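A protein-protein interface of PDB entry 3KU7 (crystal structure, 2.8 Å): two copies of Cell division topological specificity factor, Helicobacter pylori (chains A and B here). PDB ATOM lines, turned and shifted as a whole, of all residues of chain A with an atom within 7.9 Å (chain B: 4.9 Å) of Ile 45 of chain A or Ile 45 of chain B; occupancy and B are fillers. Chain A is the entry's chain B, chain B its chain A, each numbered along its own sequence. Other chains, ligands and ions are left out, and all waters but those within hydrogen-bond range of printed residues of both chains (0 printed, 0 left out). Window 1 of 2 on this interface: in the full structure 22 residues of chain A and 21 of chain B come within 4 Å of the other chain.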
ATOM      1  N   LEU A  25      35.167 -33.773  -8.179  1.00  0.00           N
ATOM      2  CA  LEU A  25      35.325 -32.400  -7.734  1.00  0.00           C
ATOM      3  C   LEU A  25      35.531 -32.270  -6.233  1.00  0.00           C
ATOM      4  O   LEU A  25      34.846 -32.909  -5.443  1.00  0.00           O
ATOM      5  CB  LEU A  25      34.108 -31.575  -8.171  1.00  0.00           C
ATOM      6  CG  LEU A  25      34.022 -30.089  -7.807  1.00  0.00           C
ATOM      7  CD1 LEU A  25      33.101 -29.384  -8.778  1.00  0.00           C
ATOM      8  CD2 LEU A  25      33.505 -29.919  -6.402  1.00  0.00           C
ATOM      9  N   LEU A  27      35.904 -29.430  -3.075  1.00  0.00           N
ATOM     10  CA  LEU A  27      35.757 -28.061  -2.608  1.00  0.00           C
ATOM     11  C   LEU A  27      36.244 -28.189  -1.187  1.00  0.00           C
ATOM     12  O   LEU A  27      35.608 -28.815  -0.346  1.00  0.00           O
ATOM     13  CB  LEU A  27      34.301 -27.590  -2.630  1.00  0.00           C
ATOM     14  CG  LEU A  27      34.118 -26.117  -3.052  1.00  0.00           C
ATOM     15  CD1 LEU A  27      32.691 -25.698  -2.893  1.00  0.00           C
ATOM     16  CD2 LEU A  27      34.953 -25.203  -2.201  1.00  0.00           C
ATOM     17  N   MET A  38      27.675 -22.615   2.149  1.00  0.00           N
ATOM     18  CA  MET A  38      28.185 -23.906   1.698  1.00  0.00           C
ATOM     19  C   MET A  38      26.861 -24.620   1.651  1.00  0.00           C
ATOM     20  O   MET A  38      25.967 -24.273   2.418  1.00  0.00           O
ATOM     21  CB  MET A  38      29.065 -24.576   2.762  1.00  0.00           C
ATOM     22  CG  MET A  38      30.497 -24.096   2.860  1.00  0.00           C
ATOM     23  SD  MET A  38      31.516 -24.505   1.404  1.00  0.00           S
ATOM     24  CE  MET A  38      31.261 -26.270   1.207  1.00  0.00           C
ATOM     25  N   GLU A  40      24.583 -25.086  -1.184  1.00  0.00           N
ATOM     26  CA  GLU A  40      23.802 -24.103  -1.924  1.00  0.00           C
ATOM     27  C   GLU A  40      24.748 -23.995  -3.077  1.00  0.00           C
ATOM     28  O   GLU A  40      24.401 -24.067  -4.254  1.00  0.00           O
ATOM     29  CB  GLU A  40      23.802 -22.763  -1.209  1.00  0.00           C
ATOM     30  CG  GLU A  40      22.454 -22.114  -1.139  1.00  0.00           C
ATOM     31  CD  GLU A  40      21.991 -21.994   0.287  1.00  0.00           C
ATOM     32  OE1 GLU A  40      22.376 -21.021   0.961  1.00  0.00           O
ATOM     33  OE2 GLU A  40      21.261 -22.891   0.747  1.00  0.00           O
ATOM     34  N   MET A  41      25.992 -23.800  -2.687  1.00  0.00           N
ATOM     35  CA  MET A  41      27.062 -23.729  -3.639  1.00  0.00           C
ATOM     36  C   MET A  41      27.103 -25.156  -4.135  1.00  0.00           C
ATOM     37  O   MET A  41      27.120 -25.421  -5.329  1.00  0.00           O
ATOM     38  CB  MET A  41      28.364 -23.402  -2.923  1.00  0.00           C
ATOM     39  CG  MET A  41      28.569 -21.949  -2.641  1.00  0.00           C
ATOM     40  SD  MET A  41      30.242 -21.555  -3.131  1.00  0.00           S
ATOM     41  CE  MET A  41      31.150 -22.138  -1.631  1.00  0.00           C
ATOM     42  N   ARG A  42      27.096 -26.079  -3.179  1.00  0.00           N
ATOM     43  CA  ARG A  42      27.151 -27.490  -3.493  1.00  0.00           C
ATOM     44  C   ARG A  42      26.012 -27.773  -4.443  1.00  0.00           C
ATOM     45  O   ARG A  42      26.217 -28.312  -5.524  1.00  0.00           O
ATOM     46  CB  ARG A  42      27.041 -28.326  -2.208  1.00  0.00           C
ATOM     47  CG  ARG A  42      27.315 -29.812  -2.390  1.00  0.00           C
ATOM     48  CD  ARG A  42      26.008 -30.578  -2.379  1.00  0.00           C
ATOM     49  NE  ARG A  42      25.341 -30.449  -1.090  1.00  0.00           N
ATOM     50  CZ  ARG A  42      24.027 -30.526  -0.920  1.00  0.00           C
ATOM     51  NH1 ARG A  42      23.227 -30.731  -1.956  1.00  0.00           N
ATOM     52  NH2 ARG A  42      23.513 -30.405   0.290  1.00  0.00           N
ATOM     53  N   LYS A  43      24.808 -27.380  -4.054  1.00  0.00           N
ATOM     54  CA  LYS A  43      23.653 -27.613  -4.905  1.00  0.00           C
ATOM     55  C   LYS A  43      23.840 -27.012  -6.291  1.00  0.00           C
ATOM     56  O   LYS A  43      23.808 -27.736  -7.287  1.00  0.00           O
ATOM     57  CB  LYS A  43      22.393 -27.068  -4.231  1.00  0.00           C
ATOM     58  CG  LYS A  43      21.910 -27.951  -3.094  1.00  0.00           C
ATOM     59  CD  LYS A  43      20.887 -27.253  -2.226  1.00  0.00           C
ATOM     60  CE  LYS A  43      20.456 -28.154  -1.095  1.00  0.00           C
ATOM     61  NZ  LYS A  43      19.722 -27.368  -0.083  1.00  0.00           N
ATOM     62  N   GLU A  44      24.049 -25.697  -6.343  1.00  0.00           N
ATOM     63  CA  GLU A  44      24.258 -24.961  -7.596  1.00  0.00           C
ATOM     64  C   GLU A  44      25.348 -25.605  -8.443  1.00  0.00           C
ATOM     65  O   GLU A  44      25.104 -26.040  -9.565  1.00  0.00           O
ATOM     66  CB  GLU A  44      24.649 -23.512  -7.286  1.00  0.00           C
ATOM     67  CG  GLU A  44      23.505 -22.509  -7.364  1.00  0.00           C
ATOM     68  CD  GLU A  44      23.469 -21.792  -8.701  1.00  0.00           C
ATOM     69  OE1 GLU A  44      23.344 -22.479  -9.742  1.00  0.00           O
ATOM     70  OE2 GLU A  44      23.573 -20.540  -8.704  1.00  0.00           O
ATOM     71  N   ILE A  45      26.551 -25.654  -7.893  1.00  0.00           N
ATOM     72  CA  ILE A  45      27.673 -26.253  -8.584  1.00  0.00           C
ATOM     73  C   ILE A  45      27.340 -27.610  -9.203  1.00  0.00           C
ATOM     74  O   ILE A  45      27.744 -27.896 -10.330  1.00  0.00           O
ATOM     75  CB  ILE A  45      28.871 -26.402  -7.634  1.00  0.00           C
ATOM     76  CG1 ILE A  45      29.433 -25.014  -7.306  1.00  0.00           C
ATOM     77  CG2 ILE A  45      29.940 -27.270  -8.275  1.00  0.00           C
ATOM     78  CD1 ILE A  45      30.492 -25.014  -6.232  1.00  0.00           C
ATOM     79  N   ILE A  46      26.610 -28.451  -8.481  1.00  0.00           N
ATOM     80  CA  ILE A  46      26.258 -29.757  -9.033  1.00  0.00           C
ATOM     81  C   ILE A  46      25.387 -29.490 -10.253  1.00  0.00           C
ATOM     82  O   ILE A  46      25.641 -30.007 -11.347  1.00  0.00           O
ATOM     83  CB  ILE A  46      25.443 -30.596  -8.034  1.00  0.00           C
ATOM     84  CG1 ILE A  46      26.247 -30.833  -6.760  1.00  0.00           C
ATOM     85  CG2 ILE A  46      25.082 -31.931  -8.642  1.00  0.00           C
ATOM     86  CD1 ILE A  46      25.414 -31.416  -5.648  1.00  0.00           C
ATOM     87  N   ALA A  47      24.383 -28.642 -10.063  1.00  0.00           N
ATOM     88  CA  ALA A  47      23.488 -28.296 -11.148  1.00  0.00           C
ATOM     89  C   ALA A  47      24.264 -27.984 -12.428  1.00  0.00           C
ATOM     90  O   ALA A  47      23.986 -28.566 -13.483  1.00  0.00           O
ATOM     91  CB  ALA A  47      22.653 -27.120 -10.756  1.00  0.00           C
ATOM     92  N   VAL A  48      25.241 -27.087 -12.331  1.00  0.00           N
ATOM     93  CA  VAL A  48      26.037 -26.695 -13.491  1.00  0.00           C
ATOM     94  C   VAL A  48      26.667 -27.904 -14.124  1.00  0.00           C
ATOM     95  O   VAL A  48      26.695 -28.065 -15.345  1.00  0.00           O
ATOM     96  CB  VAL A  48      27.163 -25.715 -13.111  1.00  0.00           C
ATOM     97  CG1 VAL A  48      28.165 -25.607 -14.270  1.00  0.00           C
ATOM     98  CG2 VAL A  48      26.562 -24.349 -12.750  1.00  0.00           C
ATOM     99  N   ILE A  49      27.204 -28.750 -13.274  1.00  0.00           N
ATOM    100  CA  ILE A  49      27.832 -29.949 -13.764  1.00  0.00           C
ATOM    101  C   ILE A  49      26.836 -30.814 -14.542  1.00  0.00           C
ATOM    102  O   ILE A  49      27.146 -31.301 -15.626  1.00  0.00           O
ATOM    103  CB  ILE A  49      28.491 -30.699 -12.584  1.00  0.00           C
ATOM    104  CG1 ILE A  49      29.643 -29.839 -12.050  1.00  0.00           C
ATOM    105  CG2 ILE A  49      29.009 -32.048 -13.021  1.00  0.00           C
ATOM    106  CD1 ILE A  49      30.233 -30.341 -10.757  1.00  0.00           C
ATOM    107  N   GLN A  50      25.630 -30.970 -14.001  1.00  0.00           N
ATOM    108  CA  GLN A  50      24.586 -31.754 -14.658  1.00  0.00           C
ATOM    109  C   GLN A  50      24.199 -31.082 -15.963  1.00  0.00           C
ATOM    110  O   GLN A  50      24.009 -31.739 -16.986  1.00  0.00           O
ATOM    111  CB  GLN A  50      23.354 -31.884 -13.757  1.00  0.00           C
ATOM    112  CG  GLN A  50      23.629 -32.588 -12.426  1.00  0.00           C
ATOM    113  CD  GLN A  50      22.452 -33.428 -11.945  1.00  0.00           C
ATOM    114  OE1 GLN A  50      22.216 -34.526 -12.458  1.00  0.00           O
ATOM    115  NE2 GLN A  50      21.702 -32.912 -10.974  1.00  0.00           N
ATOM    116  N   LYS A  51      24.094 -29.764 -15.922  1.00  0.00           N
ATOM    117  CA  LYS A  51      23.751 -29.002 -17.104  1.00  0.00           C
ATOM    118  C   LYS A  51      24.735 -29.309 -18.219  1.00  0.00           C
ATOM    119  O   LYS A  51      24.370 -29.359 -19.390  1.00  0.00           O
ATOM    120  CB  LYS A  51      23.782 -27.502 -16.779  1.00  0.00           C
ATOM    121  CG  LYS A  51      23.883 -26.562 -17.993  1.00  0.00           C
ATOM    122  CD  LYS A  51      23.338 -25.157 -17.654  1.00  0.00           C
ATOM    123  CE  LYS A  51      24.404 -24.049 -17.540  1.00  0.00           C
ATOM    124  NZ  LYS A  51      24.762 -23.482 -18.869  1.00  0.00           N
ATOM    125  N   TYR A  52      25.989 -29.520 -17.843  1.00  0.00           N
ATOM    126  CA  TYR A  52      27.007 -29.787 -18.834  1.00  0.00           C
ATOM    127  C   TYR A  52      27.364 -31.218 -19.108  1.00  0.00           C
ATOM    128  O   TYR A  52      27.795 -31.524 -20.199  1.00  0.00           O
ATOM    129  CB  TYR A  52      28.294 -29.071 -18.493  1.00  0.00           C
ATOM    130  CG  TYR A  52      28.274 -27.625 -18.814  1.00  0.00           C
ATOM    131  CD1 TYR A  52      27.878 -26.703 -17.861  1.00  0.00           C
ATOM    132  CD2 TYR A  52      28.683 -27.166 -20.064  1.00  0.00           C
ATOM    133  CE1 TYR A  52      27.900 -25.350 -18.128  1.00  0.00           C
ATOM    134  CE2 TYR A  52      28.706 -25.799 -20.351  1.00  0.00           C
ATOM    135  CZ  TYR A  52      28.309 -24.898 -19.369  1.00  0.00           C
ATOM    136  OH  TYR A  52      28.327 -23.542 -19.598  1.00  0.00           O
ATOM    137  N   ILE A  58      25.272 -39.167  -9.573  1.00  0.00           N
ATOM    138  CA  ILE A  58      26.091 -38.289  -8.760  1.00  0.00           C
ATOM    139  C   ILE A  58      26.217 -38.665  -7.295  1.00  0.00           C
ATOM    140  O   ILE A  58      25.227 -38.955  -6.625  1.00  0.00           O
ATOM    141  CB  ILE A  58      25.566 -36.869  -8.845  1.00  0.00           C
ATOM    142  CG1 ILE A  58      26.099 -36.240 -10.125  1.00  0.00           C
ATOM    143  CG2 ILE A  58      25.895 -36.100  -7.577  1.00  0.00           C
ATOM    144  CD1 ILE A  58      25.394 -35.009 -10.527  1.00  0.00           C
ATOM    145  N   VAL A  74      32.477 -34.618  -4.885  1.00  0.00           N
ATOM    146  CA  VAL A  74      31.414 -35.011  -5.784  1.00  0.00           C
ATOM    147  C   VAL A  74      32.000 -35.842  -6.915  1.00  0.00           C
ATOM    148  O   VAL A  74      32.733 -35.335  -7.751  1.00  0.00           O
ATOM    149  CB  VAL A  74      30.699 -33.781  -6.382  1.00  0.00           C
ATOM    150  CG1 VAL A  74      29.559 -34.199  -7.283  1.00  0.00           C
ATOM    151  CG2 VAL A  74      30.156 -32.924  -5.280  1.00  0.00           C
ATOM    152  N   ILE A  76      31.323 -37.816 -10.219  1.00  0.00           N
ATOM    153  CA  ILE A  76      30.350 -37.793 -11.309  1.00  0.00           C
ATOM    154  C   ILE A  76      30.661 -38.751 -12.454  1.00  0.00           C
ATOM    155  O   ILE A  76      31.754 -38.746 -13.003  1.00  0.00           O
ATOM    156  CB  ILE A  76      30.218 -36.363 -11.939  1.00  0.00           C
ATOM    157  CG1 ILE A  76      29.836 -35.323 -10.885  1.00  0.00           C
ATOM    158  CG2 ILE A  76      29.142 -36.362 -12.997  1.00  0.00           C
ATOM    159  CD1 ILE A  76      31.002 -34.652 -10.244  1.00  0.00           C
ATOM    160  N   LEU B  25      39.215 -25.502  -4.932  1.00  0.00           N
ATOM    161  CA  LEU B  25      38.385 -26.345  -5.774  1.00  0.00           C
ATOM    162  C   LEU B  25      39.196 -27.130  -6.786  1.00  0.00           C
ATOM    163  O   LEU B  25      40.007 -26.570  -7.513  1.00  0.00           O
ATOM    164  CB  LEU B  25      37.363 -25.474  -6.496  1.00  0.00           C
ATOM    165  CG  LEU B  25      36.641 -26.142  -7.645  1.00  0.00           C
ATOM    166  CD1 LEU B  25      35.485 -26.958  -7.121  1.00  0.00           C
ATOM    167  CD2 LEU B  25      36.153 -25.055  -8.559  1.00  0.00           C
ATOM    168  N   MET B  41      32.603 -25.073 -18.490  1.00  0.00           N
ATOM    169  CA  MET B  41      32.160 -25.516 -17.190  1.00  0.00           C
ATOM    170  C   MET B  41      32.984 -24.819 -16.096  1.00  0.00           C
ATOM    171  O   MET B  41      32.460 -24.390 -15.062  1.00  0.00           O
ATOM    172  CB  MET B  41      32.306 -27.026 -17.127  1.00  0.00           C
ATOM    173  CG  MET B  41      31.317 -27.707 -16.239  1.00  0.00           C
ATOM    174  SD  MET B  41      31.770 -29.433 -16.112  1.00  0.00           S
ATOM    175  CE  MET B  41      30.336 -30.129 -15.434  1.00  0.00           C
ATOM    176  N   ARG B  42      34.277 -24.688 -16.348  1.00  0.00           N
ATOM    177  CA  ARG B  42      35.179 -24.053 -15.403  1.00  0.00           C
ATOM    178  C   ARG B  42      34.629 -22.699 -15.099  1.00  0.00           C
ATOM    179  O   ARG B  42      34.327 -22.364 -13.951  1.00  0.00           O
ATOM    180  CB  ARG B  42      36.553 -23.885 -16.039  1.00  0.00           C
ATOM    181  CG  ARG B  42      37.620 -23.332 -15.124  1.00  0.00           C
ATOM    182  CD  ARG B  42      38.742 -22.770 -15.977  1.00  0.00           C
ATOM    183  NE  ARG B  42      38.263 -21.639 -16.772  1.00  0.00           N
ATOM    184  CZ  ARG B  42      38.948 -21.071 -17.763  1.00  0.00           C
ATOM    185  NH1 ARG B  42      40.145 -21.535 -18.091  1.00  0.00           N
ATOM    186  NH2 ARG B  42      38.442 -20.028 -18.415  1.00  0.00           N
ATOM    187  N   LYS B  43      34.494 -21.930 -16.171  1.00  0.00           N
ATOM    188  CA  LYS B  43      34.008 -20.574 -16.081  1.00  0.00           C
ATOM    189  C   LYS B  43      32.738 -20.466 -15.266  1.00  0.00           C
ATOM    190  O   LYS B  43      32.655 -19.625 -14.365  1.00  0.00           O
ATOM    191  CB  LYS B  43      33.777 -19.995 -17.480  1.00  0.00           C
ATOM    192  CG  LYS B  43      35.036 -19.912 -18.367  1.00  0.00           C
ATOM    193  CD  LYS B  43      34.807 -19.096 -19.665  1.00  0.00           C
ATOM    194  CE  LYS B  43      35.808 -19.445 -20.770  1.00  0.00           C
ATOM    195  NZ  LYS B  43      36.629 -18.276 -21.220  1.00  0.00           N
ATOM    196  N   GLU B  44      31.754 -21.315 -15.559  1.00  0.00           N
ATOM    197  CA  GLU B  44      30.490 -21.241 -14.828  1.00  0.00           C
ATOM    198  C   GLU B  44      30.642 -21.671 -13.374  1.00  0.00           C
ATOM    199  O   GLU B  44      30.063 -21.058 -12.477  1.00  0.00           O
ATOM    200  CB  GLU B  44      29.388 -22.059 -15.525  1.00  0.00           C
ATOM    201  CG  GLU B  44      28.137 -21.214 -15.873  1.00  0.00           C
ATOM    202  CD  GLU B  44      26.929 -22.020 -16.367  1.00  0.00           C
ATOM    203  OE1 GLU B  44      25.934 -22.185 -15.610  1.00  0.00           O
ATOM    204  OE2 GLU B  44      26.971 -22.476 -17.527  1.00  0.00           O
ATOM    205  N   ILE B  45      31.433 -22.710 -13.139  1.00  0.00           N
ATOM    206  CA  ILE B  45      31.647 -23.171 -11.779  1.00  0.00           C
ATOM    207  C   ILE B  45      32.230 -22.033 -10.954  1.00  0.00           C
ATOM    208  O   ILE B  45      31.795 -21.755  -9.835  1.00  0.00           O
ATOM    209  CB  ILE B  45      32.622 -24.323 -11.714  1.00  0.00           C
ATOM    210  CG1 ILE B  45      32.017 -25.557 -12.374  1.00  0.00           C
ATOM    211  CG2 ILE B  45      32.939 -24.608 -10.257  1.00  0.00           C
ATOM    212  CD1 ILE B  45      30.830 -26.053 -11.662  1.00  0.00           C
ATOM    213  N   ILE B  46      33.236 -21.375 -11.515  1.00  0.00           N
ATOM    214  CA  ILE B  46      33.875 -20.263 -10.822  1.00  0.00           C
ATOM    215  C   ILE B  46      32.835 -19.164 -10.609  1.00  0.00           C
ATOM    216  O   ILE B  46      32.703 -18.599  -9.522  1.00  0.00           O
ATOM    217  CB  ILE B  46      35.025 -19.646 -11.628  1.00  0.00           C
ATOM    218  CG1 ILE B  46      35.951 -20.731 -12.168  1.00  0.00           C
ATOM    219  CG2 ILE B  46      35.792 -18.679 -10.732  1.00  0.00           C
ATOM    220  CD1 ILE B  46      36.645 -21.440 -11.109  1.00  0.00           C
ATOM    221  N   ALA B  47      32.076 -18.872 -11.655  1.00  0.00           N
ATOM    222  CA  ALA B  47      31.058 -17.839 -11.557  1.00  0.00           C
ATOM    223  C   ALA B  47      30.161 -18.084 -10.345  1.00  0.00           C
ATOM    224  O   ALA B  47      29.837 -17.171  -9.597  1.00  0.00           O
ATOM    225  CB  ALA B  47      30.228 -17.811 -12.814  1.00  0.00           C
ATOM    226  N   VAL B  48      29.783 -19.334 -10.127  1.00  0.00           N
ATOM    227  CA  VAL B  48      28.914 -19.658  -9.003  1.00  0.00           C
ATOM    228  C   VAL B  48      29.595 -19.412  -7.680  1.00  0.00           C
ATOM    229  O   VAL B  48      28.998 -18.874  -6.740  1.00  0.00           O
ATOM    230  CB  VAL B  48      28.425 -21.132  -9.066  1.00  0.00           C
ATOM    231  CG1 VAL B  48      27.590 -21.467  -7.830  1.00  0.00           C
ATOM    232  CG2 VAL B  48      27.635 -21.339 -10.345  1.00  0.00           C
ATOM    233  N   ILE B  49      30.850 -19.796  -7.601  1.00  0.00           N
ATOM    234  CA  ILE B  49      31.534 -19.583  -6.360  1.00  0.00           C
ATOM    235  C   ILE B  49      31.569 -18.095  -6.049  1.00  0.00           C
ATOM    236  O   ILE B  49      31.204 -17.699  -4.948  1.00  0.00           O
ATOM    237  CB  ILE B  49      32.944 -20.194  -6.409  1.00  0.00           C
ATOM    238  CG1 ILE B  49      32.829 -21.718  -6.293  1.00  0.00           C
ATOM    239  CG2 ILE B  49      33.793 -19.639  -5.300  1.00  0.00           C
ATOM    240  CD1 ILE B  49      34.131 -22.452  -6.590  1.00  0.00           C
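OE2 of Glu 44 of chain B lies within salt-bridge range of NZ of Lys 51 of chain A (2.8 Å). The side-chain carboxylate (OE2) of Glu 44 of chain B is in hydrogen-bond range of the side-chain hydroxyl (OH) of Tyr 52 of chain A, 2.7 Å away.
The backbone NH of Leu 25 of chain A lies within hydrogen-bond range of the backbone carbonyl oxygen of Val 74 of chain A (2.9 Å).
Among the printed residues, merely in contact across the chains: Leu 25 of chain A with Leu 25 of chain B, Met 41 of chain A with Ile 49 of chain B, Glu 44 of chain A with Val 48 of chain B, Ile 45 of chain A with Ile 45 of chain B, Val 48 of chain A with Glu 44 of chain B, Val 48 of chain A with Ile 45 of chain B, Val 48 of chain A with Val 48 of chain B, Ile 49 of chain A with Met 41 of chain B, Ile 49 of chain A with Ile 45 of chain B and Tyr 52 of chain A with Met 41 of chain B.
Printed residues of chain B within 4 Å of Ile 45 of chain A: Ile 45. Printed residues of chain A within 4 Å of Ile 45 of chain B: Ile 45, Val 48 and Ile 49. Of the printed residues of chain A, Val 48 of chain B touches Glu 44 and Val 48. Of the printed residues of chain B, Lys 51 of chain A touches Glu 44. Ile 58 of chain A touches none of the printed residues of chain B. Lys 43 of chain B touches none of the printed residues of chain A. The nearest printed residue of chain A that does not touch Ile 45 of chain B is Leu 25 of chain A (5.0 Å).
Of the 19 printed residues of chain A, 8 touch a printed residue of chain B. Hydrophobic or aromatic side chains of chain A within 4 Å of the printed part of chain B: Leu 25, Met 41, Ile 45, Val 48, Ile 49 and Tyr 52. Of the 10 printed residues of chain B, 6 touch a printed residue of chain A. Hydrophobic or aromatic side chains of chain B that line the printed part of chain A: Leu 25, Met 41, Ile 45 and Val 48. Among the printed residues, 12 pairs touch across the chains.
Met 41 of chain A touches Ile 49 of chain B, and with the chains exchanged Ile 49 of chain A touches Met 41 of chain B. Glu 44 of chain A touches Val 48 of chain B, and with the chains exchanged Val 48 of chain A touches Glu 44 of chain B. Ile 45 of chain A touches its own counterpart, Ile 45 of chain B. Val 48 of chain B touches its own counterpart, Val 48 of chain A. Positions printed for both chains: 25, 41, 42, 43, 44, 45, 46, 47, 48 and 49. Of the 12 pairs that touch across the chains among the printed residues, 7 have their exchanged pair printed and touching as well.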
